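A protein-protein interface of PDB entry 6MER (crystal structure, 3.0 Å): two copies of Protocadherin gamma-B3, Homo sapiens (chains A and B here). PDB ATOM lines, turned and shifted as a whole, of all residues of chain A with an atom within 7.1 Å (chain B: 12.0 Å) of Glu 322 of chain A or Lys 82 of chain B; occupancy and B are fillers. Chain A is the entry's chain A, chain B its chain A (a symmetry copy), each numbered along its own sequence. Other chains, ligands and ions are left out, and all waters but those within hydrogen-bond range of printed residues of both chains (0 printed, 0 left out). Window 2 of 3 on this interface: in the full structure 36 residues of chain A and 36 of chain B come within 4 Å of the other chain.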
ATOM      1  N   ALA A 320     -29.906  -4.417  29.401  1.00  0.00           N
ATOM      2  CA  ALA A 320     -30.127  -5.825  29.113  1.00  0.00           C
ATOM      3  C   ALA A 320     -28.829  -6.578  29.365  1.00  0.00           C
ATOM      4  O   ALA A 320     -27.745  -6.059  29.090  1.00  0.00           O
ATOM      5  CB  ALA A 320     -30.600  -6.040  27.670  1.00  0.00           C
ATOM      6  N   SER A 321     -28.949  -7.795  29.888  1.00  0.00           N
ATOM      7  CA  SER A 321     -27.784  -8.602  30.221  1.00  0.00           C
ATOM      8  C   SER A 321     -28.207 -10.060  30.321  1.00  0.00           C
ATOM      9  O   SER A 321     -29.397 -10.385  30.320  1.00  0.00           O
ATOM     10  CB  SER A 321     -27.133  -8.127  31.524  1.00  0.00           C
ATOM     11  OG  SER A 321     -28.086  -8.065  32.570  1.00  0.00           O
ATOM     12  N   GLU A 322     -27.207 -10.941  30.407  1.00  0.00           N
ATOM     13  CA  GLU A 322     -27.441 -12.379  30.548  1.00  0.00           C
ATOM     14  C   GLU A 322     -27.780 -12.689  32.006  1.00  0.00           C
ATOM     15  O   GLU A 322     -26.992 -13.264  32.760  1.00  0.00           O
ATOM     16  CB  GLU A 322     -26.227 -13.169  30.078  1.00  0.00           C
ATOM     17  CG  GLU A 322     -25.777 -12.850  28.664  1.00  0.00           C
ATOM     18  CD  GLU A 322     -24.588 -13.686  28.229  1.00  0.00           C
ATOM     19  OE1 GLU A 322     -24.271 -14.678  28.918  1.00  0.00           O
ATOM     20  OE2 GLU A 322     -23.968 -13.351  27.197  1.00  0.00           O
ATOM     21  N   SER A 323     -28.992 -12.289  32.394  1.00  0.00           N
ATOM     22  CA  SER A 323     -29.466 -12.426  33.772  1.00  0.00           C
ATOM     23  C   SER A 323     -28.506 -11.751  34.748  1.00  0.00           C
ATOM     24  O   SER A 323     -28.298 -12.220  35.869  1.00  0.00           O
ATOM     25  CB  SER A 323     -29.684 -13.894  34.140  1.00  0.00           C
ATOM     26  OG  SER A 323     -30.675 -14.483  33.316  1.00  0.00           O
ATOM     27  N   GLN A 324     -27.932 -10.629  34.305  1.00  0.00           N
ATOM     28  CA  GLN A 324     -26.933  -9.846  35.044  1.00  0.00           C
ATOM     29  C   GLN A 324     -25.962 -10.742  35.812  1.00  0.00           C
ATOM     30  O   GLN A 324     -25.688 -10.547  36.998  1.00  0.00           O
ATOM     31  CB  GLN A 324     -27.603  -8.816  35.961  1.00  0.00           C
ATOM     32  CG  GLN A 324     -28.614  -9.354  36.966  1.00  0.00           C
ATOM     33  CD  GLN A 324     -29.655  -8.321  37.354  1.00  0.00           C
ATOM     34  OE1 GLN A 324     -29.844  -7.323  36.658  1.00  0.00           O
ATOM     35  NE2 GLN A 324     -30.337  -8.556  38.469  1.00  0.00           N
ATOM     36  N   HIS A 325     -25.424 -11.734  35.104  1.00  0.00           N
ATOM     37  CA  HIS A 325     -24.459 -12.677  35.652  1.00  0.00           C
ATOM     38  C   HIS A 325     -23.178 -12.614  34.835  1.00  0.00           C
ATOM     39  O   HIS A 325     -23.224 -12.626  33.599  1.00  0.00           O
ATOM     40  CB  HIS A 325     -25.016 -14.104  35.650  1.00  0.00           C
ATOM     41  CG  HIS A 325     -26.047 -14.354  36.707  1.00  0.00           C
ATOM     42  ND1 HIS A 325     -26.873 -15.457  36.694  1.00  0.00           N
ATOM     43  CD2 HIS A 325     -26.378 -13.650  37.815  1.00  0.00           C
ATOM     44  CE1 HIS A 325     -27.674 -15.418  37.743  1.00  0.00           C
ATOM     45  NE2 HIS A 325     -27.393 -14.332  38.440  1.00  0.00           N
ATOM     46  N   ILE A 326     -22.041 -12.549  35.522  1.00  0.00           N
ATOM     47  CA  ILE A 326     -20.730 -12.508  34.885  1.00  0.00           C
ATOM     48  C   ILE A 326     -19.904 -13.678  35.395  1.00  0.00           C
ATOM     49  O   ILE A 326     -19.919 -13.986  36.592  1.00  0.00           O
ATOM     50  CB  ILE A 326     -19.992 -11.181  35.158  1.00  0.00           C
ATOM     51  CG1 ILE A 326     -20.963 -10.001  35.147  1.00  0.00           C
ATOM     52  CG2 ILE A 326     -18.892 -10.967  34.131  1.00  0.00           C
ATOM     53  CD1 ILE A 326     -20.339  -8.718  35.650  1.00  0.00           C
ATOM     54  N   THR A 334     -15.480  -8.870  27.129  1.00  0.00           N
ATOM     55  CA  THR A 334     -16.716  -9.638  27.084  1.00  0.00           C
ATOM     56  C   THR A 334     -17.910  -8.733  27.358  1.00  0.00           C
ATOM     57  O   THR A 334     -17.942  -8.014  28.362  1.00  0.00           O
ATOM     58  CB  THR A 334     -16.671 -10.775  28.104  1.00  0.00           C
ATOM     59  OG1 THR A 334     -15.625 -11.690  27.756  1.00  0.00           O
ATOM     60  CG2 THR A 334     -17.999 -11.518  28.137  1.00  0.00           C
ATOM     61  N   ALA A 335     -18.894  -8.769  26.459  1.00  0.00           N
ATOM     62  CA  ALA A 335     -20.100  -7.962  26.607  1.00  0.00           C
ATOM     63  C   ALA A 335     -20.870  -8.370  27.857  1.00  0.00           C
ATOM     64  O   ALA A 335     -21.429  -9.469  27.920  1.00  0.00           O
ATOM     65  CB  ALA A 335     -20.986  -8.090  25.368  1.00  0.00           C
ATOM     66  N   VAL A 336     -20.900  -7.490  28.854  1.00  0.00           N
ATOM     67  CA  VAL A 336     -21.568  -7.787  30.116  1.00  0.00           C
ATOM     68  C   VAL A 336     -22.995  -7.252  30.131  1.00  0.00           C
ATOM     69  O   VAL A 336     -23.903  -7.906  30.648  1.00  0.00           O
ATOM     70  CB  VAL A 336     -20.740  -7.223  31.288  1.00  0.00           C
ATOM     71  CG1 VAL A 336     -21.518  -7.324  32.583  1.00  0.00           C
ATOM     72  CG2 VAL A 336     -19.415  -7.960  31.401  1.00  0.00           C
ATOM     73  N   ALA A 337     -23.217  -6.068  29.565  1.00  0.00           N
ATOM     74  CA  ALA A 337     -24.546  -5.479  29.530  1.00  0.00           C
ATOM     75  C   ALA A 337     -24.703  -4.668  28.254  1.00  0.00           C
ATOM     76  O   ALA A 337     -23.724  -4.167  27.694  1.00  0.00           O
ATOM     77  CB  ALA A 337     -24.804  -4.598  30.758  1.00  0.00           C
ATOM     78  N   LEU A 338     -25.946  -4.546  27.800  1.00  0.00           N
ATOM     79  CA  LEU A 338     -26.288  -3.766  26.620  1.00  0.00           C
ATOM     80  C   LEU A 338     -27.078  -2.534  27.036  1.00  0.00           C
ATOM     81  O   LEU A 338     -27.997  -2.622  27.856  1.00  0.00           O
ATOM     82  CB  LEU A 338     -27.099  -4.599  25.625  1.00  0.00           C
ATOM     83  CG  LEU A 338     -26.401  -5.838  25.063  1.00  0.00           C
ATOM     84  CD1 LEU A 338     -27.304  -6.563  24.078  1.00  0.00           C
ATOM     85  CD2 LEU A 338     -25.080  -5.457  24.410  1.00  0.00           C
ATOM     86  N   LEU A 410     -24.606  -6.401  39.011  1.00  0.00           N
ATOM     87  CA  LEU A 410     -24.002  -7.462  38.211  1.00  0.00           C
ATOM     88  C   LEU A 410     -23.298  -8.431  39.153  1.00  0.00           C
ATOM     89  O   LEU A 410     -22.285  -8.082  39.768  1.00  0.00           O
ATOM     90  CB  LEU A 410     -23.031  -6.881  37.186  1.00  0.00           C
ATOM     91  CG  LEU A 410     -23.641  -5.928  36.158  1.00  0.00           C
ATOM     92  CD1 LEU A 410     -22.551  -5.239  35.354  1.00  0.00           C
ATOM     93  CD2 LEU A 410     -24.596  -6.672  35.240  1.00  0.00           C
ATOM     94  N   GLY B  25     -29.169 -14.914  10.039  1.00  0.00           N
ATOM     95  CA  GLY B  25     -28.107 -15.898  10.110  1.00  0.00           C
ATOM     96  C   GLY B  25     -28.050 -16.666  11.410  1.00  0.00           C
ATOM     97  O   GLY B  25     -26.961 -17.048  11.850  1.00  0.00           O
ATOM     98  N   PHE B  26     -29.197 -16.904  12.042  1.00  0.00           N
ATOM     99  CA  PHE B  26     -29.270 -17.623  13.309  1.00  0.00           C
ATOM    100  C   PHE B  26     -29.744 -19.047  13.044  1.00  0.00           C
ATOM    101  O   PHE B  26     -30.886 -19.260  12.623  1.00  0.00           O
ATOM    102  CB  PHE B  26     -30.202 -16.912  14.287  1.00  0.00           C
ATOM    103  CG  PHE B  26     -29.533 -15.840  15.095  1.00  0.00           C
ATOM    104  CD1 PHE B  26     -29.290 -16.026  16.446  1.00  0.00           C
ATOM    105  CD2 PHE B  26     -29.143 -14.649  14.507  1.00  0.00           C
ATOM    106  CE1 PHE B  26     -28.673 -15.044  17.196  1.00  0.00           C
ATOM    107  CE2 PHE B  26     -28.524 -13.662  15.252  1.00  0.00           C
ATOM    108  CZ  PHE B  26     -28.289 -13.860  16.598  1.00  0.00           C
ATOM    109  N   GLY B  27     -28.867 -20.017  13.290  1.00  0.00           N
ATOM    110  CA  GLY B  27     -29.264 -21.410  13.205  1.00  0.00           C
ATOM    111  C   GLY B  27     -30.052 -21.825  14.437  1.00  0.00           C
ATOM    112  O   GLY B  27     -29.787 -21.378  15.553  1.00  0.00           O
ATOM    113  N   GLY B  29     -29.969 -24.542  15.905  1.00  0.00           N
ATOM    114  CA  GLY B  29     -29.194 -25.402  16.785  1.00  0.00           C
ATOM    115  C   GLY B  29     -28.683 -24.714  18.033  1.00  0.00           C
ATOM    116  O   GLY B  29     -28.316 -25.393  18.999  1.00  0.00           O
ATOM    117  N   ASP B  30     -28.646 -23.380  18.040  1.00  0.00           N
ATOM    118  CA  ASP B  30     -28.213 -22.613  19.202  1.00  0.00           C
ATOM    119  C   ASP B  30     -29.182 -21.472  19.492  1.00  0.00           C
ATOM    120  O   ASP B  30     -28.781 -20.417  19.989  1.00  0.00           O
ATOM    121  CB  ASP B  30     -26.794 -22.079  19.008  1.00  0.00           C
ATOM    122  CG  ASP B  30     -26.674 -21.166  17.803  1.00  0.00           C
ATOM    123  OD1 ASP B  30     -26.849 -19.939  17.965  1.00  0.00           O
ATOM    124  OD2 ASP B  30     -26.411 -21.674  16.693  1.00  0.00           O
ATOM    125  N   LEU B  31     -30.462 -21.674  19.190  1.00  0.00           N
ATOM    126  CA  LEU B  31     -31.476 -20.640  19.358  1.00  0.00           C
ATOM    127  C   LEU B  31     -31.853 -20.435  20.824  1.00  0.00           C
ATOM    128  O   LEU B  31     -31.814 -19.293  21.301  1.00  0.00           O
ATOM    129  CB  LEU B  31     -32.718 -20.972  18.525  1.00  0.00           C
ATOM    130  CG  LEU B  31     -33.754 -19.859  18.403  1.00  0.00           C
ATOM    131  CD1 LEU B  31     -33.310 -18.838  17.370  1.00  0.00           C
ATOM    132  CD2 LEU B  31     -35.109 -20.435  18.050  1.00  0.00           C
ATOM    133  N   PRO B  32     -32.225 -21.479  21.581  1.00  0.00           N
ATOM    134  CA  PRO B  32     -32.596 -21.244  22.986  1.00  0.00           C
ATOM    135  C   PRO B  32     -31.416 -20.893  23.873  1.00  0.00           C
ATOM    136  O   PRO B  32     -31.627 -20.369  24.974  1.00  0.00           O
ATOM    137  CB  PRO B  32     -33.234 -22.571  23.409  1.00  0.00           C
ATOM    138  CG  PRO B  32     -32.549 -23.576  22.572  1.00  0.00           C
ATOM    139  CD  PRO B  32     -32.329 -22.913  21.241  1.00  0.00           C
ATOM    140  N   THR B  33     -30.186 -21.164  23.436  1.00  0.00           N
ATOM    141  CA  THR B  33     -29.012 -20.823  24.230  1.00  0.00           C
ATOM    142  C   THR B  33     -28.687 -19.337  24.189  1.00  0.00           C
ATOM    143  O   THR B  33     -27.941 -18.857  25.050  1.00  0.00           O
ATOM    144  CB  THR B  33     -27.799 -21.625  23.755  1.00  0.00           C
ATOM    145  OG1 THR B  33     -27.552 -21.350  22.370  1.00  0.00           O
ATOM    146  CG2 THR B  33     -28.041 -23.117  23.935  1.00  0.00           C
ATOM    147  N   ARG B  34     -29.223 -18.600  23.216  1.00  0.00           N
ATOM    148  CA  ARG B  34     -28.975 -17.170  23.105  1.00  0.00           C
ATOM    149  C   ARG B  34     -30.100 -16.317  23.675  1.00  0.00           C
ATOM    150  O   ARG B  34     -29.919 -15.104  23.818  1.00  0.00           O
ATOM    151  CB  ARG B  34     -28.732 -16.784  21.640  1.00  0.00           C
ATOM    152  CG  ARG B  34     -27.556 -17.507  21.003  1.00  0.00           C
ATOM    153  CD  ARG B  34     -26.965 -16.704  19.855  1.00  0.00           C
ATOM    154  NE  ARG B  34     -26.391 -15.442  20.314  1.00  0.00           N
ATOM    155  CZ  ARG B  34     -25.748 -14.582  19.532  1.00  0.00           C
ATOM    156  NH1 ARG B  34     -25.589 -14.846  18.241  1.00  0.00           N
ATOM    157  NH2 ARG B  34     -25.259 -13.458  20.038  1.00  0.00           N
ATOM    158  N   ASN B  35     -31.248 -16.917  23.995  1.00  0.00           N
ATOM    159  CA  ASN B  35     -32.357 -16.243  24.670  1.00  0.00           C
ATOM    160  C   ASN B  35     -32.744 -14.949  23.946  1.00  0.00           C
ATOM    161  O   ASN B  35     -32.506 -13.836  24.413  1.00  0.00           O
ATOM    162  CB  ASN B  35     -32.007 -15.970  26.136  1.00  0.00           C
ATOM    163  CG  ASN B  35     -31.739 -17.241  26.916  1.00  0.00           C
ATOM    164  OD1 ASN B  35     -32.419 -18.251  26.734  1.00  0.00           O
ATOM    165  ND2 ASN B  35     -30.740 -17.198  27.791  1.00  0.00           N
ATOM    166  N   LEU B  36     -33.357 -15.135  22.780  1.00  0.00           N
ATOM    167  CA  LEU B  36     -33.768 -14.002  21.961  1.00  0.00           C
ATOM    168  C   LEU B  36     -34.962 -13.303  22.599  1.00  0.00           C
ATOM    169  O   LEU B  36     -36.002 -13.925  22.836  1.00  0.00           O
ATOM    170  CB  LEU B  36     -34.106 -14.468  20.548  1.00  0.00           C
ATOM    171  CG  LEU B  36     -32.947 -15.093  19.768  1.00  0.00           C
ATOM    172  CD1 LEU B  36     -33.350 -15.364  18.329  1.00  0.00           C
ATOM    173  CD2 LEU B  36     -31.718 -14.199  19.824  1.00  0.00           C
ATOM    174  N   ARG B  37     -34.809 -12.011  22.880  1.00  0.00           N
ATOM    175  CA  ARG B  37     -35.850 -11.208  23.501  1.00  0.00           C
ATOM    176  C   ARG B  37     -36.049  -9.928  22.702  1.00  0.00           C
ATOM    177  O   ARG B  37     -35.286  -9.613  21.785  1.00  0.00           O
ATOM    178  CB  ARG B  37     -35.508 -10.872  24.959  1.00  0.00           C
ATOM    179  CG  ARG B  37     -35.255 -12.084  25.837  1.00  0.00           C
ATOM    180  CD  ARG B  37     -34.920 -11.673  27.260  1.00  0.00           C
ATOM    181  NE  ARG B  37     -33.765 -10.781  27.318  1.00  0.00           N
ATOM    182  CZ  ARG B  37     -32.503 -11.195  27.349  1.00  0.00           C
ATOM    183  NH1 ARG B  37     -32.228 -12.492  27.325  1.00  0.00           N
ATOM    184  NH2 ARG B  37     -31.514 -10.313  27.404  1.00  0.00           N
ATOM    185  N   ILE B  39     -36.797  -5.901  23.654  1.00  0.00           N
ATOM    186  CA  ILE B  39     -36.938  -4.833  24.635  1.00  0.00           C
ATOM    187  C   ILE B  39     -37.637  -3.659  23.961  1.00  0.00           C
ATOM    188  O   ILE B  39     -37.188  -3.172  22.916  1.00  0.00           O
ATOM    189  CB  ILE B  39     -35.581  -4.415  25.223  1.00  0.00           C
ATOM    190  CG1 ILE B  39     -34.537  -4.236  24.117  1.00  0.00           C
ATOM    191  CG2 ILE B  39     -35.108  -5.436  26.246  1.00  0.00           C
ATOM    192  CD1 ILE B  39     -33.237  -3.639  24.605  1.00  0.00           C
ATOM    193  N   MET B  78     -33.445  -5.959  19.360  1.00  0.00           N
ATOM    194  CA  MET B  78     -33.485  -7.366  19.723  1.00  0.00           C
ATOM    195  C   MET B  78     -32.203  -7.731  20.459  1.00  0.00           C
ATOM    196  O   MET B  78     -31.107  -7.337  20.047  1.00  0.00           O
ATOM    197  CB  MET B  78     -33.650  -8.247  18.483  1.00  0.00           C
ATOM    198  CG  MET B  78     -34.007  -9.690  18.787  1.00  0.00           C
ATOM    199  SD  MET B  78     -34.058 -10.701  17.298  1.00  0.00           S
ATOM    200  CE  MET B  78     -34.956 -12.131  17.892  1.00  0.00           C
ATOM    201  N   VAL B  79     -32.342  -8.484  21.546  1.00  0.00           N
ATOM    202  CA  VAL B  79     -31.227  -8.820  22.423  1.00  0.00           C
ATOM    203  C   VAL B  79     -30.918 -10.303  22.285  1.00  0.00           C
ATOM    204  O   VAL B  79     -31.805 -11.149  22.450  1.00  0.00           O
ATOM    205  CB  VAL B  79     -31.534  -8.462  23.888  1.00  0.00           C
ATOM    206  CG1 VAL B  79     -30.310  -8.706  24.757  1.00  0.00           C
ATOM    207  CG2 VAL B  79     -31.992  -7.020  23.995  1.00  0.00           C
ATOM    208  N   ALA B  80     -29.661 -10.614  21.984  1.00  0.00           N
ATOM    209  CA  ALA B  80     -29.158 -11.976  21.973  1.00  0.00           C
ATOM    210  C   ALA B  80     -28.096 -12.124  23.055  1.00  0.00           C
ATOM    211  O   ALA B  80     -27.461 -11.148  23.462  1.00  0.00           O
ATOM    212  CB  ALA B  80     -28.576 -12.352  20.605  1.00  0.00           C
ATOM    213  N   GLU B  81     -27.912 -13.353  23.523  1.00  0.00           N
ATOM    214  CA  GLU B  81     -26.949 -13.643  24.572  1.00  0.00           C
ATOM    215  C   GLU B  81     -25.887 -14.607  24.061  1.00  0.00           C
ATOM    216  O   GLU B  81     -26.112 -15.375  23.121  1.00  0.00           O
ATOM    217  CB  GLU B  81     -27.631 -14.235  25.812  1.00  0.00           C
ATOM    218  CG  GLU B  81     -28.695 -13.342  26.426  1.00  0.00           C
ATOM    219  CD  GLU B  81     -29.346 -13.970  27.645  1.00  0.00           C
ATOM    220  OE1 GLU B  81     -28.989 -15.118  27.986  1.00  0.00           O
ATOM    221  OE2 GLU B  81     -30.211 -13.316  28.262  1.00  0.00           O
ATOM    222  N   LYS B  82     -24.719 -14.550  24.703  1.00  0.00           N
ATOM    223  CA  LYS B  82     -23.572 -15.401  24.409  1.00  0.00           C
ATOM    224  C   LYS B  82     -23.185 -15.321  22.935  1.00  0.00           C
ATOM    225  O   LYS B  82     -23.413 -16.279  22.184  1.00  0.00           O
ATOM    226  CB  LYS B  82     -23.868 -16.850  24.801  1.00  0.00           C
ATOM    227  CG  LYS B  82     -24.329 -17.016  26.240  1.00  0.00           C
ATOM    228  CD  LYS B  82     -24.785 -18.438  26.513  1.00  0.00           C
ATOM    229  CE  LYS B  82     -25.322 -18.583  27.927  1.00  0.00           C
ATOM    230  NZ  LYS B  82     -25.836 -19.957  28.187  1.00  0.00           N
ATOM    231  N   PRO B  83     -22.600 -14.202  22.477  1.00  0.00           N
ATOM    232  CA  PRO B  83     -22.349 -12.986  23.257  1.00  0.00           C
ATOM    233  C   PRO B  83     -23.540 -12.033  23.226  1.00  0.00           C
ATOM    234  O   PRO B  83     -24.497 -12.278  22.492  1.00  0.00           O
ATOM    235  CB  PRO B  83     -21.143 -12.374  22.552  1.00  0.00           C
ATOM    236  CG  PRO B  83     -21.347 -12.749  21.123  1.00  0.00           C
ATOM    237  CD  PRO B  83     -22.013 -14.110  21.128  1.00  0.00           C
ATOM    238  N   LEU B  84     -23.480 -10.962  24.012  1.00  0.00           N
ATOM    239  CA  LEU B  84     -24.536  -9.958  24.015  1.00  0.00           C
ATOM    240  C   LEU B  84     -24.381  -9.053  22.798  1.00  0.00           C
ATOM    241  O   LEU B  84     -23.337  -8.419  22.616  1.00  0.00           O
ATOM    242  CB  LEU B  84     -24.499  -9.138  25.303  1.00  0.00           C
ATOM    243  CG  LEU B  84     -25.089  -9.788  26.555  1.00  0.00           C
ATOM    244  CD1 LEU B  84     -24.911  -8.876  27.750  1.00  0.00           C
ATOM    245  CD2 LEU B  84     -26.558 -10.107  26.347  1.00  0.00           C
ATOM    246  N   ASN B  85     -25.420  -8.994  21.968  1.00  0.00           N
ATOM    247  CA  ASN B  85     -25.417  -8.159  20.777  1.00  0.00           C
ATOM    248  C   ASN B  85     -26.793  -7.541  20.588  1.00  0.00           C
ATOM    249  O   ASN B  85     -27.803  -8.079  21.049  1.00  0.00           O
ATOM    250  CB  ASN B  85     -25.025  -8.955  19.522  1.00  0.00           C
ATOM    251  CG  ASN B  85     -23.571  -9.383  19.533  1.00  0.00           C
ATOM    252  OD1 ASN B  85     -23.260 -10.570  19.435  1.00  0.00           O
ATOM    253  ND2 ASN B  85     -22.670  -8.414  19.650  1.00  0.00           N
ATOM    254  N   PHE B  86     -26.821  -6.402  19.902  1.00  0.00           N
ATOM    255  CA  PHE B  86     -28.055  -5.703  19.585  1.00  0.00           C
ATOM    256  C   PHE B  86     -28.410  -5.911  18.119  1.00  0.00           C
ATOM    257  O   PHE B  86     -27.527  -5.968  17.258  1.00  0.00           O
ATOM    258  CB  PHE B  86     -27.929  -4.207  19.884  1.00  0.00           C
ATOM    259  CG  PHE B  86     -28.510  -3.800  21.208  1.00  0.00           C
ATOM    260  CD1 PHE B  86     -29.529  -4.536  21.787  1.00  0.00           C
ATOM    261  CD2 PHE B  86     -28.038  -2.680  21.871  1.00  0.00           C
ATOM    262  CE1 PHE B  86     -30.067  -4.163  23.004  1.00  0.00           C
ATOM    263  CE2 PHE B  86     -28.571  -2.302  23.089  1.00  0.00           C
ATOM    264  CZ  PHE B  86     -29.588  -3.044  23.656  1.00  0.00           C
ATOM    265  N   PHE B  87     -29.707  -6.024  17.844  1.00  0.00           N
ATOM    266  CA  PHE B  87     -30.218  -6.203  16.486  1.00  0.00           C
ATOM    267  C   PHE B  87     -31.392  -5.248  16.295  1.00  0.00           C
ATOM    268  O   PHE B  87     -32.496  -5.505  16.782  1.00  0.00           O
ATOM    269  CB  PHE B  87     -30.631  -7.651  16.236  1.00  0.00           C
ATOM    270  CG  PHE B  87     -29.487  -8.625  16.292  1.00  0.00           C
ATOM    271  CD1 PHE B  87     -28.712  -8.867  15.169  1.00  0.00           C
ATOM    272  CD2 PHE B  87     -29.187  -9.296  17.465  1.00  0.00           C
ATOM    273  CE1 PHE B  87     -27.659  -9.761  15.218  1.00  0.00           C
ATOM    274  CE2 PHE B  87     -28.135 -10.190  17.519  1.00  0.00           C
ATOM    275  CZ  PHE B  87     -27.371 -10.423  16.393  1.00  0.00           C
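Val 79 of chain B touches Ala 320 of chain A (CG1 to CB, 3.96 Å). O of Ser 321 of chain A touches NH2 of Arg 37 of chain B, at 3.6 Å. CD1 of Leu 84 of chain B touches CA of Ser 321 of chain A (3.8 Å). Glu 81 of chain B touches Glu 322 of chain A. CD2 of Leu 84 of chain B touches CG of Glu 322 of chain A (3.7 Å). Ala 335 of chain A touches Leu 84 of chain B (O to CD1, 3.5 Å). Val 336 of chain A touches Leu 84 of chain B. Leu 84 of chain B touches Ala 337 of chain A. Val 79 of chain B touches Leu 338 of chain A. Phe 86 of chain B touches Leu 338 of chain A (CZ to CB, 3.5 Å).
Glu 322 of chain A touches just these residues of chain B: Glu 81 (3.7 Å), Lys 82 (2.9 Å) and Leu 84 (3.7 Å). Lys 82 of chain B touches one residue of chain A. Ala 320 of chain A touches just one residue of chain B: Val 79 (3.96 Å). Ser 321 of chain A touches three residues of chain B. Of chain B, only Leu 84 (3.5 Å) comes within 4 Å of Ala 335 of chain A. Of the printed residues of chain A, Val 79 of chain B touches Ala 320 and Leu 338. Printed residues of chain B within 4 Å of Leu 338 of chain A: Val 79, Leu 84, Asn 85 and Phe 86. Printed residues of chain A within 4 Å of Leu 84 of chain B: Ser 321 (3.8 Å), Glu 322 (3.7 Å), Ala 335 (3.5 Å), Val 336 (3.2 Å), Ala 337 (3.7 Å) and Leu 338 (3.8 Å). Of the printed residues of chain B, Val 336 of chain A touches Leu 84. Gln 324 of chain A touches none of the printed residues of chain B. Ile 326 of chain A touches none of the printed residues of chain B. The nearest residue of chain B that does not touch Glu 322 of chain A is Pro 83 of chain B (4.2 Å). The nearest printed residue of chain A that does not touch Asn 85 of chain B is Ala 335 of chain A (5.7 Å).
O of Ala 320 of chain A is in hydrogen-bond range of N of Leu 338 of chain A, at 2.7 Å. OG of Ser 321 of chain A is in hydrogen-bond range of N of Gln 324 of chain A, at 3.1 Å. O of Asn 35 of chain B sits at hydrogen-bond distance from NH1 of Arg 37 of chain B (3.2 Å). ND2 of Asn 35 of chain B is in hydrogen-bond range of OE1 of Glu 81 of chain B, 2.7 Å away. The guanidinium group (NH2) of Arg 37 of chain B is in salt-bridge range of the side-chain carboxylate (OE2) of Glu 81 of chain B (3.4 Å). O of Asn 85 of chain B sits at hydrogen-bond distance from N of Ala 80 of chain B, at 3.3 Å.
No position is printed for both chains.
Of the 13 printed residues of chain A, 7 touch a printed residue of chain B. Hydrophobic or aromatic side chains of chain A within 4 Å of the printed part of chain B: Ala 320, Ala 335 and Leu 338. Of the 23 printed residues of chain B, 7 touch a printed residue of chain A.
OE2 of Glu 322 of chain A is in hydrogen-bond range of N of Lys 82 of chain B (2.9 Å).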
